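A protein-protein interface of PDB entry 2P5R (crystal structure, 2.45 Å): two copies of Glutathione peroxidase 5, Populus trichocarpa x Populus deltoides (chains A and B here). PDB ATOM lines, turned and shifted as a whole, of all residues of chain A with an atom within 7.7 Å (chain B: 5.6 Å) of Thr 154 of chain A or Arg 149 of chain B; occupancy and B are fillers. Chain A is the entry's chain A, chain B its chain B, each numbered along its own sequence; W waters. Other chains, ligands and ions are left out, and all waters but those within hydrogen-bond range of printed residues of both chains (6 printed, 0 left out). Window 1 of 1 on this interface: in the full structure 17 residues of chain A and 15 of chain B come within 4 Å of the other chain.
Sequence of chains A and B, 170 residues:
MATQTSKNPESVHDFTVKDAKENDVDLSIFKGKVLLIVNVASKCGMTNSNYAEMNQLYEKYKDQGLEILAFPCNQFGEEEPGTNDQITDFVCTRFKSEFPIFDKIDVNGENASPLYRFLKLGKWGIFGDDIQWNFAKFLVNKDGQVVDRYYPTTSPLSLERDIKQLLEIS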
ATOM      1  N   ASN A  50      17.317  21.573 -13.042  1.00  0.00           N
ATOM      2  CA  ASN A  50      17.747  20.688 -14.122  1.00  0.00           C
ATOM      3  C   ASN A  50      17.403  19.215 -13.865  1.00  0.00           C
ATOM      4  O   ASN A  50      16.956  18.509 -14.774  1.00  0.00           O
ATOM      5  CB  ASN A  50      19.259  20.843 -14.354  1.00  0.00           C
ATOM      6  CG  ASN A  50      19.591  21.972 -15.322  1.00  0.00           C
ATOM      7  OD1 ASN A  50      19.462  21.820 -16.537  1.00  0.00           O
ATOM      8  ND2 ASN A  50      20.012  23.111 -14.786  1.00  0.00           N
ATOM      9  N   GLU A  53      13.719  18.261 -14.578  1.00  0.00           N
ATOM     10  CA  GLU A  53      13.462  18.289 -16.006  1.00  0.00           C
ATOM     11  C   GLU A  53      14.079  17.098 -16.746  1.00  0.00           C
ATOM     12  O   GLU A  53      13.444  16.528 -17.646  1.00  0.00           O
ATOM     13  CB  GLU A  53      13.941  19.622 -16.588  1.00  0.00           C
ATOM     14  CG  GLU A  53      13.325  20.819 -15.870  1.00  0.00           C
ATOM     15  CD  GLU A  53      13.300  22.067 -16.715  1.00  0.00           C
ATOM     16  OE1 GLU A  53      12.875  23.127 -16.202  1.00  0.00           O
ATOM     17  OE2 GLU A  53      13.700  21.990 -17.897  1.00  0.00           O
ATOM     18  N   ASP A 129      34.277  25.802 -26.917  1.00  0.00           N
ATOM     19  CA  ASP A 129      34.255  26.537 -25.658  1.00  0.00           C
ATOM     20  C   ASP A 129      34.378  25.635 -24.441  1.00  0.00           C
ATOM     21  O   ASP A 129      33.858  24.525 -24.434  1.00  0.00           O
ATOM     22  CB  ASP A 129      32.952  27.329 -25.529  1.00  0.00           C
ATOM     23  CG  ASP A 129      32.755  28.316 -26.656  1.00  0.00           C
ATOM     24  OD1 ASP A 129      31.639  28.356 -27.213  1.00  0.00           O
ATOM     25  OD2 ASP A 129      33.709  29.049 -26.980  1.00  0.00           O
ATOM     26  N   GLN A 132      30.978  26.172 -19.523  1.00  0.00           N
ATOM     27  CA  GLN A 132      30.743  27.431 -18.830  1.00  0.00           C
ATOM     28  C   GLN A 132      30.367  27.329 -17.370  1.00  0.00           C
ATOM     29  O   GLN A 132      30.727  28.197 -16.586  1.00  0.00           O
ATOM     30  CB  GLN A 132      29.666  28.247 -19.553  1.00  0.00           C
ATOM     31  CG  GLN A 132      30.002  28.553 -20.981  1.00  0.00           C
ATOM     32  CD  GLN A 132      29.703  27.397 -21.895  1.00  0.00           C
ATOM     33  OE1 GLN A 132      29.447  26.277 -21.447  1.00  0.00           O
ATOM     34  NE2 GLN A 132      29.743  27.655 -23.192  1.00  0.00           N
ATOM     35  N   PHE A 135      25.831  21.927 -15.536  1.00  0.00           N
ATOM     36  CA  PHE A 135      24.695  21.662 -16.403  1.00  0.00           C
ATOM     37  C   PHE A 135      24.738  22.135 -17.857  1.00  0.00           C
ATOM     38  O   PHE A 135      23.744  22.632 -18.381  1.00  0.00           O
ATOM     39  CB  PHE A 135      23.425  22.182 -15.710  1.00  0.00           C
ATOM     40  CG  PHE A 135      23.243  21.644 -14.310  1.00  0.00           C
ATOM     41  CD1 PHE A 135      22.833  20.334 -14.101  1.00  0.00           C
ATOM     42  CD2 PHE A 135      23.525  22.436 -13.201  1.00  0.00           C
ATOM     43  CE1 PHE A 135      22.708  19.816 -12.807  1.00  0.00           C
ATOM     44  CE2 PHE A 135      23.404  21.928 -11.904  1.00  0.00           C
ATOM     45  CZ  PHE A 135      22.997  20.620 -11.707  1.00  0.00           C
ATOM     46  N   ALA A 136      25.885  21.997 -18.510  1.00  0.00           N
ATOM     47  CA  ALA A 136      25.956  22.349 -19.921  1.00  0.00           C
ATOM     48  C   ALA A 136      25.408  21.081 -20.591  1.00  0.00           C
ATOM     49  O   ALA A 136      25.486  19.998 -20.002  1.00  0.00           O
ATOM     50  CB  ALA A 136      27.390  22.598 -20.336  1.00  0.00           C
ATOM     51  N   LYS A 137      24.843  21.198 -21.790  1.00  0.00           N
ATOM     52  CA  LYS A 137      24.293  20.020 -22.454  1.00  0.00           C
ATOM     53  C   LYS A 137      24.841  19.766 -23.857  1.00  0.00           C
ATOM     54  O   LYS A 137      25.186  20.697 -24.588  1.00  0.00           O
ATOM     55  CB  LYS A 137      22.759  20.102 -22.553  1.00  0.00           C
ATOM     56  CG  LYS A 137      21.974  20.188 -21.231  1.00  0.00           C
ATOM     57  CD  LYS A 137      21.930  21.624 -20.696  1.00  0.00           C
ATOM     58  CE  LYS A 137      20.936  21.771 -19.534  1.00  0.00           C
ATOM     59  NZ  LYS A 137      20.892  23.160 -18.973  1.00  0.00           N
ATOM     60  N   ARG A 149      24.927  21.535 -28.760  1.00  0.00           N
ATOM     61  CA  ARG A 149      25.475  21.967 -27.490  1.00  0.00           C
ATOM     62  C   ARG A 149      24.584  23.087 -26.960  1.00  0.00           C
ATOM     63  O   ARG A 149      24.106  23.931 -27.714  1.00  0.00           O
ATOM     64  CB  ARG A 149      26.922  22.466 -27.622  1.00  0.00           C
ATOM     65  CG  ARG A 149      27.525  22.877 -26.258  1.00  0.00           C
ATOM     66  CD  ARG A 149      29.015  23.222 -26.308  1.00  0.00           C
ATOM     67  NE  ARG A 149      29.468  23.786 -25.036  1.00  0.00           N
ATOM     68  CZ  ARG A 149      30.737  24.034 -24.722  1.00  0.00           C
ATOM     69  NH1 ARG A 149      31.705  23.767 -25.591  1.00  0.00           N
ATOM     70  NH2 ARG A 149      31.039  24.567 -23.542  1.00  0.00           N
ATOM     71  N   TYR A 150      24.357  23.084 -25.656  1.00  0.00           N
ATOM     72  CA  TYR A 150      23.510  24.092 -25.044  1.00  0.00           C
ATOM     73  C   TYR A 150      24.197  24.717 -23.846  1.00  0.00           C
ATOM     74  O   TYR A 150      25.005  24.076 -23.173  1.00  0.00           O
ATOM     75  CB  TYR A 150      22.177  23.463 -24.627  1.00  0.00           C
ATOM     76  CG  TYR A 150      21.518  22.662 -25.733  1.00  0.00           C
ATOM     77  CD1 TYR A 150      21.950  21.384 -26.044  1.00  0.00           C
ATOM     78  CD2 TYR A 150      20.489  23.211 -26.497  1.00  0.00           C
ATOM     79  CE1 TYR A 150      21.381  20.669 -27.086  1.00  0.00           C
ATOM     80  CE2 TYR A 150      19.910  22.511 -27.543  1.00  0.00           C
ATOM     81  CZ  TYR A 150      20.360  21.239 -27.838  1.00  0.00           C
ATOM     82  OH  TYR A 150      19.814  20.553 -28.906  1.00  0.00           O
ATOM     83  N   TYR A 151      23.891  25.985 -23.599  1.00  0.00           N
ATOM     84  CA  TYR A 151      24.456  26.692 -22.463  1.00  0.00           C
ATOM     85  C   TYR A 151      23.777  26.148 -21.224  1.00  0.00           C
ATOM     86  O   TYR A 151      22.649  25.663 -21.291  1.00  0.00           O
ATOM     87  CB  TYR A 151      24.218  28.203 -22.587  1.00  0.00           C
ATOM     88  CG  TYR A 151      25.249  28.875 -23.444  1.00  0.00           C
ATOM     89  CD1 TYR A 151      25.223  28.741 -24.831  1.00  0.00           C
ATOM     90  CD2 TYR A 151      26.343  29.519 -22.866  1.00  0.00           C
ATOM     91  CE1 TYR A 151      26.271  29.215 -25.621  1.00  0.00           C
ATOM     92  CE2 TYR A 151      27.392  29.997 -23.645  1.00  0.00           C
ATOM     93  CZ  TYR A 151      27.349  29.833 -25.020  1.00  0.00           C
ATOM     94  OH  TYR A 151      28.400  30.252 -25.793  1.00  0.00           O
ATOM     95  N   PRO A 152      24.463  26.204 -20.076  1.00  0.00           N
ATOM     96  CA  PRO A 152      23.900  25.705 -18.815  1.00  0.00           C
ATOM     97  C   PRO A 152      22.483  26.227 -18.594  1.00  0.00           C
ATOM     98  O   PRO A 152      21.599  25.489 -18.166  1.00  0.00           O
ATOM     99  CB  PRO A 152      24.880  26.235 -17.772  1.00  0.00           C
ATOM    100  CG  PRO A 152      26.198  26.215 -18.521  1.00  0.00           C
ATOM    101  CD  PRO A 152      25.804  26.785 -19.866  1.00  0.00           C
ATOM    102  N   THR A 153      22.283  27.499 -18.923  1.00  0.00           N
ATOM    103  CA  THR A 153      20.998  28.171 -18.752  1.00  0.00           C
ATOM    104  C   THR A 153      19.838  27.609 -19.557  1.00  0.00           C
ATOM    105  O   THR A 153      18.689  27.899 -19.257  1.00  0.00           O
ATOM    106  CB  THR A 153      21.111  29.663 -19.084  1.00  0.00           C
ATOM    107  OG1 THR A 153      21.447  29.816 -20.471  1.00  0.00           O
ATOM    108  CG2 THR A 153      22.189  30.320 -18.215  1.00  0.00           C
ATOM    109  N   THR A 154      20.121  26.821 -20.586  1.00  0.00           N
ATOM    110  CA  THR A 154      19.045  26.248 -21.390  1.00  0.00           C
ATOM    111  C   THR A 154      18.448  25.056 -20.653  1.00  0.00           C
ATOM    112  O   THR A 154      19.115  24.044 -20.479  1.00  0.00           O
ATOM    113  CB  THR A 154      19.555  25.783 -22.789  1.00  0.00           C
ATOM    114  OG1 THR A 154      19.958  26.925 -23.561  1.00  0.00           O
ATOM    115  CG2 THR A 154      18.458  25.030 -23.543  1.00  0.00           C
ATOM    116  N   SER A 155      17.198  25.178 -20.211  1.00  0.00           N
ATOM    117  CA  SER A 155      16.554  24.084 -19.485  1.00  0.00           C
ATOM    118  C   SER A 155      16.407  22.876 -20.389  1.00  0.00           C
ATOM    119  O   SER A 155      16.232  23.006 -21.596  1.00  0.00           O
ATOM    120  CB  SER A 155      15.174  24.493 -18.968  1.00  0.00           C
ATOM    121  OG  SER A 155      14.222  24.511 -20.012  1.00  0.00           O
ATOM    122  N   PRO A 156      16.480  21.677 -19.805  1.00  0.00           N
ATOM    123  CA  PRO A 156      16.362  20.422 -20.544  1.00  0.00           C
ATOM    124  C   PRO A 156      15.164  20.356 -21.466  1.00  0.00           C
ATOM    125  O   PRO A 156      15.301  20.051 -22.651  1.00  0.00           O
ATOM    126  CB  PRO A 156      16.298  19.379 -19.436  1.00  0.00           C
ATOM    127  CG  PRO A 156      17.209  19.973 -18.386  1.00  0.00           C
ATOM    128  CD  PRO A 156      16.762  21.425 -18.379  1.00  0.00           C
ATOM    129  N   LEU A 157      13.990  20.640 -20.916  1.00  0.00           N
ATOM    130  CA  LEU A 157      12.747  20.603 -21.674  1.00  0.00           C
ATOM    131  C   LEU A 157      12.831  21.362 -23.002  1.00  0.00           C
ATOM    132  O   LEU A 157      12.121  21.044 -23.956  1.00  0.00           O
ATOM    133  CB  LEU A 157      11.620  21.167 -20.813  1.00  0.00           C
ATOM    134  CG  LEU A 157      11.404  20.476 -19.454  1.00  0.00           C
ATOM    135  CD1 LEU A 157      10.446  21.309 -18.615  1.00  0.00           C
ATOM    136  CD2 LEU A 157      10.861  19.060 -19.650  1.00  0.00           C
ATOM    137  N   SER A 158      13.702  22.363 -23.066  1.00  0.00           N
ATOM    138  CA  SER A 158      13.862  23.138 -24.286  1.00  0.00           C
ATOM    139  C   SER A 158      14.694  22.400 -25.330  1.00  0.00           C
ATOM    140  O   SER A 158      14.968  22.937 -26.396  1.00  0.00           O
ATOM    141  CB  SER A 158      14.513  24.484 -23.982  1.00  0.00           C
ATOM    142  OG  SER A 158      13.626  25.323 -23.257  1.00  0.00           O
ATOM    143  N   LEU A 159      15.092  21.172 -25.018  1.00  0.00           N
ATOM    144  CA  LEU A 159      15.883  20.376 -25.941  1.00  0.00           C
ATOM    145  C   LEU A 159      15.032  19.252 -26.496  1.00  0.00           C
ATOM    146  O   LEU A 159      15.510  18.424 -27.273  1.00  0.00           O
ATOM    147  CB  LEU A 159      17.097  19.757 -25.232  1.00  0.00           C
ATOM    148  CG  LEU A 159      18.338  20.581 -24.866  1.00  0.00           C
ATOM    149  CD1 LEU A 159      17.983  21.661 -23.869  1.00  0.00           C
ATOM    150  CD2 LEU A 159      19.394  19.651 -24.278  1.00  0.00           C
ATOM    151  N   LYS B 120      27.302  39.469 -24.042  1.00  0.00           N
ATOM    152  CA  LYS B 120      28.285  38.512 -23.560  1.00  0.00           C
ATOM    153  C   LYS B 120      28.502  38.503 -22.052  1.00  0.00           C
ATOM    154  O   LYS B 120      29.100  37.568 -21.528  1.00  0.00           O
ATOM    155  CB  LYS B 120      29.628  38.766 -24.237  1.00  0.00           C
ATOM    156  CG  LYS B 120      29.669  38.481 -25.724  1.00  0.00           C
ATOM    157  CD  LYS B 120      31.061  38.772 -26.250  1.00  0.00           C
ATOM    158  CE  LYS B 120      31.225  38.366 -27.694  1.00  0.00           C
ATOM    159  NZ  LYS B 120      32.582  38.724 -28.187  1.00  0.00           N
ATOM    160  N   PHE B 127      27.607  33.589 -20.651  1.00  0.00           N
ATOM    161  CA  PHE B 127      27.515  33.886 -22.070  1.00  0.00           C
ATOM    162  C   PHE B 127      28.746  34.604 -22.580  1.00  0.00           C
ATOM    163  O   PHE B 127      28.751  35.105 -23.697  1.00  0.00           O
ATOM    164  CB  PHE B 127      26.275  34.750 -22.337  1.00  0.00           C
ATOM    165  CG  PHE B 127      24.980  34.098 -21.937  1.00  0.00           C
ATOM    166  CD1 PHE B 127      23.835  34.863 -21.744  1.00  0.00           C
ATOM    167  CD2 PHE B 127      24.900  32.718 -21.754  1.00  0.00           C
ATOM    168  CE1 PHE B 127      22.623  34.262 -21.373  1.00  0.00           C
ATOM    169  CE2 PHE B 127      23.693  32.110 -21.384  1.00  0.00           C
ATOM    170  CZ  PHE B 127      22.556  32.885 -21.193  1.00  0.00           C
ATOM    171  N   GLY B 128      29.794  34.638 -21.766  1.00  0.00           N
ATOM    172  CA  GLY B 128      31.007  35.332 -22.149  1.00  0.00           C
ATOM    173  C   GLY B 128      31.822  34.807 -23.315  1.00  0.00           C
ATOM    174  O   GLY B 128      32.790  35.447 -23.699  1.00  0.00           O
ATOM    175  N   ASP B 129      31.463  33.664 -23.884  1.00  0.00           N
ATOM    176  CA  ASP B 129      32.229  33.120 -25.008  1.00  0.00           C
ATOM    177  C   ASP B 129      32.162  33.987 -26.263  1.00  0.00           C
ATOM    178  O   ASP B 129      31.262  34.791 -26.420  1.00  0.00           O
ATOM    179  CB  ASP B 129      31.721  31.726 -25.384  1.00  0.00           C
ATOM    180  CG  ASP B 129      31.798  30.749 -24.243  1.00  0.00           C
ATOM    181  OD1 ASP B 129      32.915  30.529 -23.736  1.00  0.00           O
ATOM    182  OD2 ASP B 129      30.741  30.197 -23.863  1.00  0.00           O
ATOM    183  N   ASP B 130      33.130  33.814 -27.154  1.00  0.00           N
ATOM    184  CA  ASP B 130      33.147  34.530 -28.420  1.00  0.00           C
ATOM    185  C   ASP B 130      32.058  33.889 -29.262  1.00  0.00           C
ATOM    186  O   ASP B 130      31.842  32.677 -29.170  1.00  0.00           O
ATOM    187  CB  ASP B 130      34.469  34.310 -29.162  1.00  0.00           C
ATOM    188  CG  ASP B 130      35.549  35.295 -28.772  1.00  0.00           C
ATOM    189  OD1 ASP B 130      36.656  35.165 -29.323  1.00  0.00           O
ATOM    190  OD2 ASP B 130      35.307  36.190 -27.937  1.00  0.00           O
ATOM    191  N   ILE B 131      31.377  34.686 -30.082  1.00  0.00           N
ATOM    192  CA  ILE B 131      30.355  34.126 -30.958  1.00  0.00           C
ATOM    193  C   ILE B 131      31.118  33.066 -31.740  1.00  0.00           C
ATOM    194  O   ILE B 131      32.127  33.362 -32.376  1.00  0.00           O
ATOM    195  CB  ILE B 131      29.775  35.193 -31.904  1.00  0.00           C
ATOM    196  CG1 ILE B 131      28.693  36.006 -31.193  1.00  0.00           C
ATOM    197  CG2 ILE B 131      29.105  34.521 -33.084  1.00  0.00           C
ATOM    198  CD1 ILE B 131      29.058  36.508 -29.837  1.00  0.00           C
ATOM    199  N   GLN B 132      30.645  31.828 -31.676  1.00  0.00           N
ATOM    200  CA  GLN B 132      31.334  30.721 -32.322  1.00  0.00           C
ATOM    201  C   GLN B 132      31.321  30.718 -33.842  1.00  0.00           C
ATOM    202  O   GLN B 132      32.298  30.318 -34.480  1.00  0.00           O
ATOM    203  CB  GLN B 132      30.776  29.392 -31.799  1.00  0.00           C
ATOM    204  CG  GLN B 132      30.920  29.193 -30.289  1.00  0.00           C
ATOM    205  CD  GLN B 132      29.892  29.984 -29.477  1.00  0.00           C
ATOM    206  OE1 GLN B 132      29.058  30.694 -30.029  1.00  0.00           O
ATOM    207  NE2 GLN B 132      29.953  29.852 -28.164  1.00  0.00           N
ATOM    208  N   ALA B 136      24.578  32.694 -34.186  1.00  0.00           N
ATOM    209  CA  ALA B 136      24.540  32.389 -32.764  1.00  0.00           C
ATOM    210  C   ALA B 136      23.242  33.090 -32.326  1.00  0.00           C
ATOM    211  O   ALA B 136      22.940  34.192 -32.805  1.00  0.00           O
ATOM    212  CB  ALA B 136      25.741  32.981 -32.059  1.00  0.00           C
ATOM    213  N   LYS B 137      22.461  32.457 -31.456  1.00  0.00           N
ATOM    214  CA  LYS B 137      21.205  33.062 -31.026  1.00  0.00           C
ATOM    215  C   LYS B 137      21.208  33.544 -29.590  1.00  0.00           C
ATOM    216  O   LYS B 137      21.777  32.907 -28.703  1.00  0.00           O
ATOM    217  CB  LYS B 137      20.030  32.094 -31.208  1.00  0.00           C
ATOM    218  CG  LYS B 137      19.673  31.741 -32.649  1.00  0.00           C
ATOM    219  CD  LYS B 137      20.568  30.640 -33.188  1.00  0.00           C
ATOM    220  CE  LYS B 137      20.067  30.139 -34.541  1.00  0.00           C
ATOM    221  NZ  LYS B 137      20.911  29.050 -35.108  1.00  0.00           N
ATOM    222  N   PHE B 138      20.550  34.679 -29.382  1.00  0.00           N
ATOM    223  CA  PHE B 138      20.420  35.296 -28.072  1.00  0.00           C
ATOM    224  C   PHE B 138      18.950  35.632 -27.826  1.00  0.00           C
ATOM    225  O   PHE B 138      18.238  36.041 -28.747  1.00  0.00           O
ATOM    226  CB  PHE B 138      21.228  36.594 -28.020  1.00  0.00           C
ATOM    227  CG  PHE B 138      22.667  36.416 -27.616  1.00  0.00           C
ATOM    228  CD1 PHE B 138      23.004  36.170 -26.294  1.00  0.00           C
ATOM    229  CD2 PHE B 138      23.686  36.552 -28.550  1.00  0.00           C
ATOM    230  CE1 PHE B 138      24.336  36.072 -25.908  1.00  0.00           C
ATOM    231  CE2 PHE B 138      25.025  36.453 -28.171  1.00  0.00           C
ATOM    232  CZ  PHE B 138      25.351  36.215 -26.853  1.00  0.00           C
ATOM    233  N   LEU B 139      18.494  35.442 -26.592  1.00  0.00           N
ATOM    234  CA  LEU B 139      17.124  35.787 -26.234  1.00  0.00           C
ATOM    235  C   LEU B 139      17.189  36.828 -25.143  1.00  0.00           C
ATOM    236  O   LEU B 139      17.880  36.650 -24.140  1.00  0.00           O
ATOM    237  CB  LEU B 139      16.334  34.589 -25.735  1.00  0.00           C
ATOM    238  CG  LEU B 139      15.773  33.659 -26.806  1.00  0.00           C
ATOM    239  CD1 LEU B 139      14.710  32.764 -26.171  1.00  0.00           C
ATOM    240  CD2 LEU B 139      15.164  34.477 -27.945  1.00  0.00           C
ATOM    241  N   VAL B 147      18.594  36.660 -21.440  1.00  0.00           N
ATOM    242  CA  VAL B 147      18.089  35.452 -20.794  1.00  0.00           C
ATOM    243  C   VAL B 147      18.726  34.143 -21.264  1.00  0.00           C
ATOM    244  O   VAL B 147      19.152  33.330 -20.444  1.00  0.00           O
ATOM    245  CB  VAL B 147      16.554  35.326 -20.991  1.00  0.00           C
ATOM    246  CG1 VAL B 147      16.012  34.161 -20.173  1.00  0.00           C
ATOM    247  CG2 VAL B 147      15.873  36.607 -20.582  1.00  0.00           C
ATOM    248  N   ASP B 148      18.776  33.936 -22.579  1.00  0.00           N
ATOM    249  CA  ASP B 148      19.336  32.710 -23.143  1.00  0.00           C
ATOM    250  C   ASP B 148      20.362  32.936 -24.244  1.00  0.00           C
ATOM    251  O   ASP B 148      20.476  34.025 -24.800  1.00  0.00           O
ATOM    252  CB  ASP B 148      18.219  31.840 -23.710  1.00  0.00           C
ATOM    253  CG  ASP B 148      17.172  31.493 -22.679  1.00  0.00           C
ATOM    254  OD1 ASP B 148      16.450  32.408 -22.241  1.00  0.00           O
ATOM    255  OD2 ASP B 148      17.078  30.301 -22.306  1.00  0.00           O
ATOM    256  N   ARG B 149      21.104  31.881 -24.553  1.00  0.00           N
ATOM    257  CA  ARG B 149      22.117  31.912 -25.596  1.00  0.00           C
ATOM    258  C   ARG B 149      22.173  30.521 -26.184  1.00  0.00           C
ATOM    259  O   ARG B 149      22.110  29.530 -25.452  1.00  0.00           O
ATOM    260  CB  ARG B 149      23.493  32.266 -25.034  1.00  0.00           C
ATOM    261  CG  ARG B 149      24.350  33.038 -26.033  1.00  0.00           C
ATOM    262  CD  ARG B 149      25.671  32.389 -26.341  1.00  0.00           C
ATOM    263  NE  ARG B 149      26.789  33.288 -26.075  1.00  0.00           N
ATOM    264  CZ  ARG B 149      27.928  33.300 -26.761  1.00  0.00           C
ATOM    265  NH1 ARG B 149      28.115  32.468 -27.771  1.00  0.00           N
ATOM    266  NH2 ARG B 149      28.887  34.142 -26.429  1.00  0.00           N
ATOM    267  N   TYR B 150      22.276  30.436 -27.505  1.00  0.00           N
ATOM    268  CA  TYR B 150      22.331  29.133 -28.140  1.00  0.00           C
ATOM    269  C   TYR B 150      23.466  29.076 -29.134  1.00  0.00           C
ATOM    270  O   TYR B 150      23.876  30.092 -29.678  1.00  0.00           O
ATOM    271  CB  TYR B 150      21.008  28.829 -28.842  1.00  0.00           C
ATOM    272  CG  TYR B 150      19.793  29.082 -27.975  1.00  0.00           C
ATOM    273  CD1 TYR B 150      19.392  30.382 -27.675  1.00  0.00           C
ATOM    274  CD2 TYR B 150      19.041  28.027 -27.468  1.00  0.00           C
ATOM    275  CE1 TYR B 150      18.276  30.625 -26.896  1.00  0.00           C
ATOM    276  CE2 TYR B 150      17.917  28.261 -26.681  1.00  0.00           C
ATOM    277  CZ  TYR B 150      17.538  29.564 -26.401  1.00  0.00           C
ATOM    278  OH  TYR B 150      16.430  29.820 -25.627  1.00  0.00           O
ATOM    279  N   TYR B 151      23.992  27.884 -29.349  1.00  0.00           N
ATOM    280  CA  TYR B 151      25.066  27.704 -30.298  1.00  0.00           C
ATOM    281  C   TYR B 151      24.514  27.829 -31.720  1.00  0.00           C
ATOM    282  O   TYR B 151      23.334  27.552 -31.975  1.00  0.00           O
ATOM    283  CB  TYR B 151      25.721  26.335 -30.084  1.00  0.00           C
ATOM    284  CG  TYR B 151      26.741  26.352 -28.975  1.00  0.00           C
ATOM    285  CD1 TYR B 151      28.084  26.628 -29.240  1.00  0.00           C
ATOM    286  CD2 TYR B 151      26.354  26.184 -27.647  1.00  0.00           C
ATOM    287  CE1 TYR B 151      29.015  26.743 -28.204  1.00  0.00           C
ATOM    288  CE2 TYR B 151      27.276  26.300 -26.600  1.00  0.00           C
ATOM    289  CZ  TYR B 151      28.602  26.584 -26.887  1.00  0.00           C
ATOM    290  OH  TYR B 151      29.492  26.760 -25.858  1.00  0.00           O
ATOM    291  N   ASP B 162      11.333  28.255 -25.581  1.00  0.00           N
ATOM    292  CA  ASP B 162      11.825  29.337 -24.743  1.00  0.00           C
ATOM    293  C   ASP B 162      11.208  30.663 -25.182  1.00  0.00           C
ATOM    294  O   ASP B 162      10.957  31.537 -24.353  1.00  0.00           O
ATOM    295  CB  ASP B 162      13.360  29.396 -24.792  1.00  0.00           C
ATOM    296  CG  ASP B 162      14.015  28.139 -24.219  1.00  0.00           C
ATOM    297  OD1 ASP B 162      13.640  27.724 -23.105  1.00  0.00           O
ATOM    298  OD2 ASP B 162      14.908  27.564 -24.874  1.00  0.00           O
HETATM  299  O   HOH W   1      35.401  30.671 -25.025  1.00  0.00           O
HETATM  300  O   HOH W   2      16.336  29.488 -19.976  1.00  0.00           O
HETATM  301  O   HOH W   3      15.151  27.327 -21.022  1.00  0.00           O
HETATM  302  O   HOH W   4      22.390  25.910 -28.162  1.00  0.00           O
HETATM  303  O   HOH W   5      21.881  27.065 -25.408  1.00  0.00           O
HETATM  304  O   HOH W   6      19.960  29.692 -22.549  1.00  0.00           O
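Of the 17 printed residues of chain B, 7 touch a printed residue of chain A.
Hydrophobic or aromatic side chains of chain B that line the printed part of chain A: Phe 127, Tyr 150 and Tyr 151.
Hydrophobic or aromatic side chains of chain A within 4 Å of the printed part of chain B: Tyr 151.
Among the printed residues, 15 pairs touch across the chains.
Among the printed residues, no Asp or Glu carboxylate lies within 4 Å of a Lys or Arg side-chain nitrogen of the other chain.
Thr 154 of chain A touches just these residues of chain B: Arg 149 and Tyr 150.
Printed residues of chain A within 4 Å of Phe 127 of chain B: Tyr 151 and Thr 153.
Arg 149 of chain B touches just these residues of chain A: Tyr 151 and Thr 154.
Of the printed residues of chain A, Tyr 151 of chain B touches Asp 129, Gln 132, Arg 149 and Tyr 151.
The nearest residue of chain B that does not touch Thr 154 of chain A is Asp 162 of chain B (4.6 Å).
The nearest residue of chain A that does not touch Arg 149 of chain B is Thr 153 of chain A (4.6 Å).
Asp 129 of chain A touches Tyr 151 of chain B, and with the chains exchanged Tyr 151 of chain A touches Asp 129 of chain B.
Arg 149 of chain A touches Tyr 151 of chain B, and with the chains exchanged Tyr 151 of chain A touches Arg 149 of chain B.
Water W1 bridges OD1 of Asp 129 of chain B and OD2 of Asp 129 of chain A.
The side-chain amino group (NZ) of Lys 137 of chain A lies within hydrogen-bond range of the backbone carbonyl oxygen (O) of Thr 154 of chain A, 2.5 Å away.
The side-chain carboxylate (OD1) of Asp 129 of chain A lies within hydrogen-bond range of the side-chain amide nitrogen (NE2) of Gln 132 of chain B, at 2.4 Å.
The side-chain hydroxyl (OH) of Tyr 151 of chain A is in hydrogen-bond range of the side-chain amide nitrogen (NE2) of Gln 132 of chain B (2.9 Å).
The side-chain carboxylate (OD1) of Asp 162 of chain B is in hydrogen-bond range of the side-chain hydroxyl (OG) of Ser 158 of chain A.
OD2 of Asp 129 of chain B is in hydrogen-bond range of NE2 of Gln 132 of chain A (2.8 Å).
The side-chain carboxylate (OD1) of Asp 129 of chain A sits at hydrogen-bond distance from the side-chain hydroxyl (OH) of Tyr 151 of chain B, 3.0 Å away.
The guanidinium group of Arg 149 of chain A lies within hydrogen-bond range of the side-chain hydroxyl of Tyr 151 of chain B.
The side-chain hydroxyl (OH) of Tyr 151 of chain A is in hydrogen-bond range of the side-chain carboxylate (OD2) of Asp 129 of chain B, at 3.0 Å.
NE2 of Gln 132 of chain A lies within hydrogen-bond range of OH of Tyr 151 of chain B, 2.8 Å away.
The side-chain hydroxyl (OH) of Tyr 151 of chain A lies within hydrogen-bond range of the guanidinium group (NH1) of Arg 149 of chain B (3.0 Å).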
